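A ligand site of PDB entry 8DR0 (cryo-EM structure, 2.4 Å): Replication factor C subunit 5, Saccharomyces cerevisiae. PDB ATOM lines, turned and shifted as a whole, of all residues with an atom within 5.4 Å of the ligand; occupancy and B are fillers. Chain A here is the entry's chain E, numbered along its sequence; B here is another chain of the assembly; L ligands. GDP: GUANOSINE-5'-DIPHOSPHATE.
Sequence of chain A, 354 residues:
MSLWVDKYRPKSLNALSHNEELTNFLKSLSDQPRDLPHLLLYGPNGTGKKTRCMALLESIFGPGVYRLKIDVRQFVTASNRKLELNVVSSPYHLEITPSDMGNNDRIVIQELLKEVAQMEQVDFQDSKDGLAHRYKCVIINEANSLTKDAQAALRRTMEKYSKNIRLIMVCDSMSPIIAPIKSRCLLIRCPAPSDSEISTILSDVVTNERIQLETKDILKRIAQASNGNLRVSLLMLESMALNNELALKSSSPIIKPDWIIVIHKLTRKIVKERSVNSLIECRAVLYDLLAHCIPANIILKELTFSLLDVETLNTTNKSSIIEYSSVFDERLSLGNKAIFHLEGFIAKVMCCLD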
ATOM      1  N   VAL A   5      -2.794   9.546   1.984  1.00  0.00           N
ATOM      2  CA  VAL A   5      -2.072   9.067   3.151  1.00  0.00           C
ATOM      3  C   VAL A   5      -1.955  10.170   4.198  1.00  0.00           C
ATOM      4  O   VAL A   5      -1.997   9.908   5.403  1.00  0.00           O
ATOM      5  CB  VAL A   5      -0.691   8.522   2.741  1.00  0.00           C
ATOM      6  CG1 VAL A   5       0.191   9.629   2.177  1.00  0.00           C
ATOM      7  CG2 VAL A   5      -0.015   7.851   3.936  1.00  0.00           C
ATOM      8  N   ASP A   6      -1.802  11.420   3.756  1.00  0.00           N
ATOM      9  CA  ASP A   6      -1.656  12.553   4.669  1.00  0.00           C
ATOM     10  C   ASP A   6      -2.990  13.207   5.005  1.00  0.00           C
ATOM     11  O   ASP A   6      -3.156  13.706   6.136  1.00  0.00           O
ATOM     12  CB  ASP A   6      -0.725  13.605   4.063  1.00  0.00           C
ATOM     13  CG  ASP A   6       0.661  13.067   3.806  1.00  0.00           C
ATOM     14  OD1 ASP A   6       1.081  12.124   4.521  1.00  0.00           O
ATOM     15  OD2 ASP A   6       1.349  13.586   2.899  1.00  0.00           O
ATOM     16  N   TYR A   8      -5.958  11.967   5.522  1.00  0.00           N
ATOM     17  CA  TYR A   8      -6.787  11.229   6.461  1.00  0.00           C
ATOM     18  C   TYR A   8      -5.998  10.686   7.651  1.00  0.00           C
ATOM     19  O   TYR A   8      -6.438   9.731   8.296  1.00  0.00           O
ATOM     20  CB  TYR A   8      -7.509  10.085   5.740  1.00  0.00           C
ATOM     21  CG  TYR A   8      -8.399  10.566   4.610  1.00  0.00           C
ATOM     22  CD1 TYR A   8      -9.598  11.208   4.873  1.00  0.00           C
ATOM     23  CD2 TYR A   8      -8.037  10.367   3.280  1.00  0.00           C
ATOM     24  CE1 TYR A   8     -10.410  11.640   3.849  1.00  0.00           C
ATOM     25  CE2 TYR A   8      -8.848  10.799   2.256  1.00  0.00           C
ATOM     26  CZ  TYR A   8     -10.034  11.437   2.547  1.00  0.00           C
ATOM     27  OH  TYR A   8     -10.845  11.869   1.523  1.00  0.00           O
ATOM     28  N   ARG A   9      -4.853  11.274   7.943  1.00  0.00           N
ATOM     29  CA  ARG A   9      -4.061  10.828   9.087  1.00  0.00           C
ATOM     30  C   ARG A   9      -4.763  11.229  10.385  1.00  0.00           C
ATOM     31  O   ARG A   9      -5.126  12.403  10.554  1.00  0.00           O
ATOM     32  CB  ARG A   9      -2.663  11.439   9.048  1.00  0.00           C
ATOM     33  CG  ARG A   9      -1.806  11.099  10.256  1.00  0.00           C
ATOM     34  CD  ARG A   9      -0.327  11.291   9.957  1.00  0.00           C
ATOM     35  NE  ARG A   9      -0.014  12.665   9.553  1.00  0.00           N
ATOM     36  CZ  ARG A   9       0.347  13.032   8.332  1.00  0.00           C
ATOM     37  NH1 ARG A   9       0.481  12.157   7.352  1.00  0.00           N
ATOM     38  NH2 ARG A   9       0.597  14.318   8.098  1.00  0.00           N
ATOM     39  N   PRO A  10      -4.988  10.297  11.317  1.00  0.00           N
ATOM     40  CA  PRO A  10      -5.656  10.658  12.565  1.00  0.00           C
ATOM     41  C   PRO A  10      -4.874  11.700  13.350  1.00  0.00           C
ATOM     42  O   PRO A  10      -3.637  11.731  13.324  1.00  0.00           O
ATOM     43  CB  PRO A  10      -5.735   9.327  13.338  1.00  0.00           C
ATOM     44  CG  PRO A  10      -5.580   8.270  12.308  1.00  0.00           C
ATOM     45  CD  PRO A  10      -4.699   8.853  11.253  1.00  0.00           C
ATOM     46  N   ALA A  15      -9.074   8.912  17.521  1.00  0.00           N
ATOM     47  CA  ALA A  15      -9.207   8.741  16.073  1.00  0.00           C
ATOM     48  C   ALA A  15      -8.440   7.541  15.536  1.00  0.00           C
ATOM     49  O   ALA A  15      -8.569   7.224  14.353  1.00  0.00           O
ATOM     50  CB  ALA A  15      -8.737  10.014  15.360  1.00  0.00           C
ATOM     51  N   LEU A  16      -7.640   6.874  16.367  1.00  0.00           N
ATOM     52  CA  LEU A  16      -6.922   5.689  15.934  1.00  0.00           C
ATOM     53  C   LEU A  16      -7.901   4.547  15.672  1.00  0.00           C
ATOM     54  O   LEU A  16      -8.924   4.423  16.357  1.00  0.00           O
ATOM     55  CB  LEU A  16      -5.894   5.271  16.973  1.00  0.00           C
ATOM     56  CG  LEU A  16      -4.927   6.367  17.442  1.00  0.00           C
ATOM     57  CD1 LEU A  16      -4.082   5.873  18.600  1.00  0.00           C
ATOM     58  CD2 LEU A  16      -4.042   6.839  16.294  1.00  0.00           C
ATOM     59  N   SER A  17      -7.590   3.724  14.677  1.00  0.00           N
ATOM     60  CA  SER A  17      -8.509   2.666  14.232  1.00  0.00           C
ATOM     61  C   SER A  17      -7.876   1.281  14.231  1.00  0.00           C
ATOM     62  O   SER A  17      -8.506   0.339  13.746  1.00  0.00           O
ATOM     63  CB  SER A  17      -9.041   2.988  12.836  1.00  0.00           C
ATOM     64  OG  SER A  17      -8.054   3.642  12.045  1.00  0.00           O
ATOM     65  N   HIS A  18      -6.653   1.129  14.745  1.00  0.00           N
ATOM     66  CA  HIS A  18      -6.043  -0.196  14.825  1.00  0.00           C
ATOM     67  C   HIS A  18      -5.155  -0.263  16.048  1.00  0.00           C
ATOM     68  O   HIS A  18      -4.673   0.755  16.557  1.00  0.00           O
ATOM     69  CB  HIS A  18      -5.257  -0.524  13.543  1.00  0.00           C
ATOM     70  CG  HIS A  18      -3.938   0.174  13.433  1.00  0.00           C
ATOM     71  ND1 HIS A  18      -2.774  -0.341  13.958  1.00  0.00           N
ATOM     72  CD2 HIS A  18      -3.586   1.331  12.834  1.00  0.00           C
ATOM     73  CE1 HIS A  18      -1.766   0.476  13.704  1.00  0.00           C
ATOM     74  NE2 HIS A  18      -2.237   1.507  13.024  1.00  0.00           N
ATOM     75  N   PRO A  44       7.758  -1.898  13.383  1.00  0.00           N
ATOM     76  CA  PRO A  44       7.986  -1.922  11.937  1.00  0.00           C
ATOM     77  C   PRO A  44       7.664  -0.591  11.292  1.00  0.00           C
ATOM     78  O   PRO A  44       6.809   0.165  11.748  1.00  0.00           O
ATOM     79  CB  PRO A  44       7.043  -3.028  11.442  1.00  0.00           C
ATOM     80  CG  PRO A  44       6.724  -3.843  12.643  1.00  0.00           C
ATOM     81  CD  PRO A  44       6.766  -2.911  13.808  1.00  0.00           C
ATOM     82  N   ASN A  45       8.367  -0.304  10.199  1.00  0.00           N
ATOM     83  CA  ASN A  45       8.205   0.976   9.508  1.00  0.00           C
ATOM     84  C   ASN A  45       6.797   1.100   8.932  1.00  0.00           C
ATOM     85  O   ASN A  45       6.164   0.110   8.548  1.00  0.00           O
ATOM     86  CB  ASN A  45       9.245   1.107   8.393  1.00  0.00           C
ATOM     87  CG  ASN A  45      10.601   1.542   8.905  1.00  0.00           C
ATOM     88  OD1 ASN A  45      10.699   2.338   9.837  1.00  0.00           O
ATOM     89  ND2 ASN A  45      11.659   1.016   8.302  1.00  0.00           N
ATOM     90  N   GLY A  46       6.319   2.339   8.866  1.00  0.00           N
ATOM     91  CA  GLY A  46       5.024   2.617   8.270  1.00  0.00           C
ATOM     92  C   GLY A  46       3.850   1.995   9.007  1.00  0.00           C
ATOM     93  O   GLY A  46       2.876   1.590   8.371  1.00  0.00           O
ATOM     94  N   THR A  47       3.929   1.921  10.333  1.00  0.00           N
ATOM     95  CA  THR A  47       2.870   1.337  11.138  1.00  0.00           C
ATOM     96  C   THR A  47       1.995   2.378  11.828  1.00  0.00           C
ATOM     97  O   THR A  47       0.818   2.108  12.092  1.00  0.00           O
ATOM     98  CB  THR A  47       3.461   0.406  12.199  1.00  0.00           C
ATOM     99  OG1 THR A  47       3.900  -0.807  11.568  1.00  0.00           O
ATOM    100  CG2 THR A  47       2.448   0.071  13.276  1.00  0.00           C
ATOM    101  N   GLY A  48       2.540   3.560  12.111  1.00  0.00           N
ATOM    102  CA  GLY A  48       1.782   4.601  12.804  1.00  0.00           C
ATOM    103  C   GLY A  48       2.436   5.028  14.102  1.00  0.00           C
ATOM    104  O   GLY A  48       1.752   5.511  15.011  1.00  0.00           O
ATOM    105  N   LYS A  49       3.762   4.860  14.201  1.00  0.00           N
ATOM    106  CA  LYS A  49       4.460   5.235  15.420  1.00  0.00           C
ATOM    107  C   LYS A  49       4.468   6.750  15.609  1.00  0.00           C
ATOM    108  O   LYS A  49       4.153   7.249  16.692  1.00  0.00           O
ATOM    109  CB  LYS A  49       5.889   4.693  15.393  1.00  0.00           C
ATOM    110  CG  LYS A  49       5.974   3.178  15.243  1.00  0.00           C
ATOM    111  CD  LYS A  49       7.386   2.668  15.458  1.00  0.00           C
ATOM    112  CE  LYS A  49       8.327   3.096  14.337  1.00  0.00           C
ATOM    113  NZ  LYS A  49       7.926   2.539  13.013  1.00  0.00           N
ATOM    114  N   LYS A  50       4.835   7.498  14.570  1.00  0.00           N
ATOM    115  CA  LYS A  50       4.839   8.952  14.671  1.00  0.00           C
ATOM    116  C   LYS A  50       3.427   9.492  14.866  1.00  0.00           C
ATOM    117  O   LYS A  50       3.218  10.453  15.619  1.00  0.00           O
ATOM    118  CB  LYS A  50       5.483   9.564  13.431  1.00  0.00           C
ATOM    119  CG  LYS A  50       5.641  11.085  13.488  1.00  0.00           C
ATOM    120  CD  LYS A  50       6.451  11.534  14.701  1.00  0.00           C
ATOM    121  CE  LYS A  50       6.741  13.025  14.676  1.00  0.00           C
ATOM    122  NZ  LYS A  50       7.663  13.395  13.566  1.00  0.00           N
ATOM    123  N   THR A  51       2.441   8.889  14.199  1.00  0.00           N
ATOM    124  CA  THR A  51       1.054   9.297  14.383  1.00  0.00           C
ATOM    125  C   THR A  51       0.635   9.126  15.845  1.00  0.00           C
ATOM    126  O   THR A  51       0.011  10.011  16.427  1.00  0.00           O
ATOM    127  CB  THR A  51       0.137   8.480  13.470  1.00  0.00           C
ATOM    128  OG1 THR A  51       0.483   8.728  12.095  1.00  0.00           O
ATOM    129  CG2 THR A  51      -1.319   8.849  13.701  1.00  0.00           C
ATOM    130  N   ARG A  52       0.984   7.990  16.452  1.00  0.00           N
ATOM    131  CA  ARG A  52       0.624   7.751  17.843  1.00  0.00           C
ATOM    132  C   ARG A  52       1.381   8.680  18.780  1.00  0.00           C
ATOM    133  O   ARG A  52       0.827   9.127  19.787  1.00  0.00           O
ATOM    134  CB  ARG A  52       0.885   6.291  18.198  1.00  0.00           C
ATOM    135  CG  ARG A  52      -0.337   5.414  18.001  1.00  0.00           C
ATOM    136  CD  ARG A  52       0.046   3.959  17.798  1.00  0.00           C
ATOM    137  NE  ARG A  52      -1.110   3.152  17.406  1.00  0.00           N
ATOM    138  CZ  ARG A  52      -1.705   3.212  16.222  1.00  0.00           C
ATOM    139  NH1 ARG A  52      -1.276   4.030  15.271  1.00  0.00           N
ATOM    140  NH2 ARG A  52      -2.758   2.441  15.991  1.00  0.00           N
ATOM    141  N   VAL A 170      11.696   7.286  18.542  1.00  0.00           N
ATOM    142  CA  VAL A 170      10.973   6.378  17.659  1.00  0.00           C
ATOM    143  C   VAL A 170      11.986   5.623  16.824  1.00  0.00           C
ATOM    144  O   VAL A 170      12.910   6.222  16.261  1.00  0.00           O
ATOM    145  CB  VAL A 170       9.975   7.139  16.761  1.00  0.00           C
ATOM    146  CG1 VAL A 170       9.106   6.157  15.996  1.00  0.00           C
ATOM    147  CG2 VAL A 170       9.127   8.079  17.595  1.00  0.00           C
ATOM    148  N   ILE A 201      -9.353   0.610   6.682  1.00  0.00           N
ATOM    149  CA  ILE A 201      -8.851   1.961   6.450  1.00  0.00           C
ATOM    150  C   ILE A 201      -8.918   2.305   4.959  1.00  0.00           C
ATOM    151  O   ILE A 201      -9.333   3.410   4.583  1.00  0.00           O
ATOM    152  CB  ILE A 201      -7.423   2.107   7.009  1.00  0.00           C
ATOM    153  CG1 ILE A 201      -7.436   1.997   8.528  1.00  0.00           C
ATOM    154  CG2 ILE A 201      -6.812   3.427   6.573  1.00  0.00           C
ATOM    155  CD1 ILE A 201      -6.076   1.706   9.134  1.00  0.00           C
ATOM    156  N   LEU A 230       1.234   0.400   6.401  1.00  0.00           N
ATOM    157  CA  LEU A 230       0.011   1.143   6.109  1.00  0.00           C
ATOM    158  C   LEU A 230       0.270   2.313   5.171  1.00  0.00           C
ATOM    159  O   LEU A 230      -0.537   2.589   4.265  1.00  0.00           O
ATOM    160  CB  LEU A 230      -0.622   1.632   7.414  1.00  0.00           C
ATOM    161  CG  LEU A 230      -2.024   2.222   7.334  1.00  0.00           C
ATOM    162  CD1 LEU A 230      -3.009   1.227   6.740  1.00  0.00           C
ATOM    163  CD2 LEU A 230      -2.487   2.658   8.711  1.00  0.00           C
ATOM    164  N   ARG A 231       1.391   3.016   5.351  1.00  0.00           N
ATOM    165  CA  ARG A 231       1.729   4.104   4.429  1.00  0.00           C
ATOM    166  C   ARG A 231       1.885   3.586   3.015  1.00  0.00           C
ATOM    167  O   ARG A 231       1.375   4.196   2.059  1.00  0.00           O
ATOM    168  CB  ARG A 231       3.012   4.791   4.889  1.00  0.00           C
ATOM    169  CG  ARG A 231       3.643   5.709   3.846  1.00  0.00           C
ATOM    170  CD  ARG A 231       4.784   6.526   4.411  1.00  0.00           C
ATOM    171  NE  ARG A 231       5.846   5.680   4.958  1.00  0.00           N
ATOM    172  CZ  ARG A 231       6.190   5.608   6.239  1.00  0.00           C
ATOM    173  NH1 ARG A 231       5.576   6.331   7.170  1.00  0.00           N
ATOM    174  NH2 ARG A 231       7.185   4.804   6.597  1.00  0.00           N
ATOM    175  N   LEU A 234      -1.589   2.768   1.539  1.00  0.00           N
ATOM    176  CA  LEU A 234      -2.347   3.958   1.138  1.00  0.00           C
ATOM    177  C   LEU A 234      -1.769   4.572  -0.132  1.00  0.00           C
ATOM    178  O   LEU A 234      -2.524   4.931  -1.047  1.00  0.00           O
ATOM    179  CB  LEU A 234      -2.345   4.982   2.275  1.00  0.00           C
ATOM    180  CG  LEU A 234      -3.262   4.647   3.457  1.00  0.00           C
ATOM    181  CD1 LEU A 234      -2.754   5.298   4.734  1.00  0.00           C
ATOM    182  CD2 LEU A 234      -4.693   5.066   3.164  1.00  0.00           C
ATOM    183  N   SER B 695       4.259  12.458   6.874  1.00  0.00           N
ATOM    184  CA  SER B 695       4.624  11.778   8.119  1.00  0.00           C
ATOM    185  C   SER B 695       5.578  10.660   7.743  1.00  0.00           C
ATOM    186  O   SER B 695       5.152   9.525   7.489  1.00  0.00           O
ATOM    187  CB  SER B 695       3.384  11.256   8.838  1.00  0.00           C
ATOM    188  OG  SER B 695       3.709  10.789  10.137  1.00  0.00           O
ATOM    189  N   THR B 696       6.871  10.972   7.718  1.00  0.00           N
ATOM    190  CA  THR B 696       7.884  10.009   7.284  1.00  0.00           C
ATOM    191  C   THR B 696       9.253  10.649   7.453  1.00  0.00           C
ATOM    192  O   THR B 696       9.373  11.847   7.708  1.00  0.00           O
ATOM    193  CB  THR B 696       7.672   9.583   5.826  1.00  0.00           C
ATOM    194  OG1 THR B 696       8.551   8.493   5.512  1.00  0.00           O
ATOM    195  CG2 THR B 696       7.947  10.747   4.886  1.00  0.00           C
ATOM    196  N   TYR B 705       6.901   7.843  -0.945  1.00  0.00           N
ATOM    197  CA  TYR B 705       6.119   9.006  -1.356  1.00  0.00           C
ATOM    198  C   TYR B 705       6.380   9.378  -2.816  1.00  0.00           C
ATOM    199  O   TYR B 705       5.438   9.616  -3.578  1.00  0.00           O
ATOM    200  CB  TYR B 705       6.423  10.187  -0.445  1.00  0.00           C
ATOM    201  CG  TYR B 705       5.501  10.300   0.756  1.00  0.00           C
ATOM    202  CD1 TYR B 705       4.290  10.969   0.651  1.00  0.00           C
ATOM    203  CD2 TYR B 705       5.847   9.738   1.969  1.00  0.00           C
ATOM    204  CE1 TYR B 705       3.447  11.073   1.740  1.00  0.00           C
ATOM    205  CE2 TYR B 705       5.010   9.837   3.065  1.00  0.00           C
ATOM    206  CZ  TYR B 705       3.809  10.504   2.950  1.00  0.00           C
ATOM    207  OH  TYR B 705       2.977  10.605   4.030  1.00  0.00           O
HETATM  208  PB  GDP L   1       5.736   5.194  11.254  1.00  0.00           P
HETATM  209  O1B GDP L   1       5.975   3.915  12.009  1.00  0.00           O
HETATM  210  O2B GDP L   1       5.998   6.378  12.159  1.00  0.00           O
HETATM  211  O3B GDP L   1       6.677   5.264  10.071  1.00  0.00           O
HETATM  212  O3A GDP L   1       4.173   5.223  10.735  1.00  0.00           O
HETATM  213  PA  GDP L   1       3.352   6.577  10.309  1.00  0.00           P
HETATM  214  O1A GDP L   1       3.008   7.367  11.551  1.00  0.00           O
HETATM  215  O2A GDP L   1       4.196   7.435   9.396  1.00  0.00           O
HETATM  216  O5' GDP L   1       1.968   6.130   9.545  1.00  0.00           O
HETATM  217  C5' GDP L   1       1.872   6.265   8.156  1.00  0.00           C
HETATM  218  C4' GDP L   1       0.446   6.611   7.775  1.00  0.00           C
HETATM  219  O4' GDP L   1      -0.545   5.466   8.321  1.00  0.00           O
HETATM  220  C3' GDP L   1       0.080   7.731   8.324  1.00  0.00           C
HETATM  221  O3' GDP L   1       0.261   8.868   7.359  1.00  0.00           O
HETATM  222  C2' GDP L   1      -1.423   7.567   8.643  1.00  0.00           C
HETATM  223  O2' GDP L   1      -2.168   8.131   7.668  1.00  0.00           O
HETATM  224  C1' GDP L   1      -1.667   6.049   8.671  1.00  0.00           C
HETATM  225  N9  GDP L   1      -2.025   5.598  10.039  1.00  0.00           N
HETATM  226  C8  GDP L   1      -1.228   5.280  11.068  1.00  0.00           C
HETATM  227  N7  GDP L   1      -2.028   4.924  12.088  1.00  0.00           N
HETATM  228  C5  GDP L   1      -3.292   5.017  11.687  1.00  0.00           C
HETATM  229  C6  GDP L   1      -4.625   4.743  12.397  1.00  0.00           C
HETATM  230  O6  GDP L   1      -4.623   4.376  13.521  1.00  0.00           O
HETATM  231  N1  GDP L   1      -5.858   4.937  11.705  1.00  0.00           N
HETATM  232  C2  GDP L   1      -5.847   5.384  10.335  1.00  0.00           C
HETATM  233  N2  GDP L   1      -7.096   5.572   9.625  1.00  0.00           N
HETATM  234  N3  GDP L   1      -4.574   5.634   9.659  1.00  0.00           N
HETATM  235  C4  GDP L   1      -3.292   5.444  10.384  1.00  0.00           C
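The guanidinium group (NH1) of Arg 52 sits at hydrogen-bond distance from a nitrogen (N7) of the ligand, 3.4 Å away.
The backbone NH (N) of Thr 47 sits at hydrogen-bond distance from an oxygen (O1B) of the ligand.
The backbone carbonyl oxygen of Val 5 sits at hydrogen-bond distance from an oxygen (O2') of the ligand, at 2.9 Å.
The backbone NH (N) of Lys 50 is in hydrogen-bond range of an oxygen (O2B) of the ligand (2.9 Å).
The guanidinium group of Arg 9 is in hydrogen-bond range of an oxygen (O3') of the ligand (3.3 Å).
An oxygen (O2A) of the ligand is in salt-bridge range of the guanidinium group (NH1) of Arg 231, at 2.8 Å.
An oxygen (O2A) of the ligand sits close to the backbone carbonyl oxygen (O) of Ser 695 of chain B, at 3.0 Å.
The backbone NH (N) of Gly 48 lies within hydrogen-bond range of an oxygen (O3A) of the ligand, at 2.7 Å.
N of Lys 49 sits at hydrogen-bond distance from O1B of the ligand (3.3 Å).
O2A of the ligand is in hydrogen-bond range of OG of Ser 695 of chain B, at 3.5 Å.
The side-chain hydroxyl (OG) of Ser 17 is in hydrogen-bond range of a nitrogen (N1) of the ligand, 2.6 Å away.
The backbone NH of Ser 17 is in hydrogen-bond range of an oxygen (O6) of the ligand (3.3 Å).
O3B of the ligand lies within hydrogen-bond range of N of Gly 46 (3.2 Å).
The side-chain amino group (NZ) of Lys 49 lies within salt-bridge range of an oxygen (O1B) of the ligand, at 2.6 Å.
The side-chain hydroxyl (OG1) of Thr 51 lies within hydrogen-bond range of an oxygen (O1A) of the ligand (2.9 Å).
The backbone NH (N) of Thr 51 lies within hydrogen-bond range of an oxygen (O1A) of the ligand, at 3.1 Å.
Merely in contact with the ligand: Leu 230, His 18, Pro 10, Leu 16, Ile 201 and Pro 44.
Hydrophobic or aromatic side chains within 4 Å of the ligand: Val 5, Pro 10, Leu 16, His 18, Ile 201 and Leu 230.
Within 4 Å of the ligand: Val 5, Arg 9, Pro 10, Leu 16, Ser 17, His 18, Pro 44, Gly 46, Thr 47, Gly 48, Lys 49, Lys 50, Thr 51, Arg 52, Ile 201, Leu 230, Arg 231 and Ser 695 of chain B.
The nearest printed residue that does not touch the ligand is Leu 234 (4.1 Å).
O of His 18 lies within hydrogen-bond range of NH2 of Arg 52, 2.6 Å away.
The backbone carbonyl oxygen (O) of Gly 48 is in hydrogen-bond range of the guanidinium group (NH1) of Arg 52, at 3.4 Å.
The guanidinium group of Arg 9 lies within salt-bridge range of the side-chain carboxylate of Asp 6, 2.9 Å away.
O of Gly 46 is in hydrogen-bond range of N of Leu 230.
The guanidinium group (NH1) of Arg 231 is in hydrogen-bond range of the backbone carbonyl oxygen (O) of Ser 695 of chain B (3.2 Å).
A ring nitrogen (NE2) of His 18 lies within hydrogen-bond range of the backbone carbonyl oxygen of Thr 47, 3.3 Å away.
OG1 of Thr 47 lies within hydrogen-bond range of O of Pro 44, 3.1 Å away.
The backbone carbonyl oxygen (O) of Pro 44 sits at hydrogen-bond distance from the side-chain amino group (NZ) of Lys 49 (2.9 Å).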
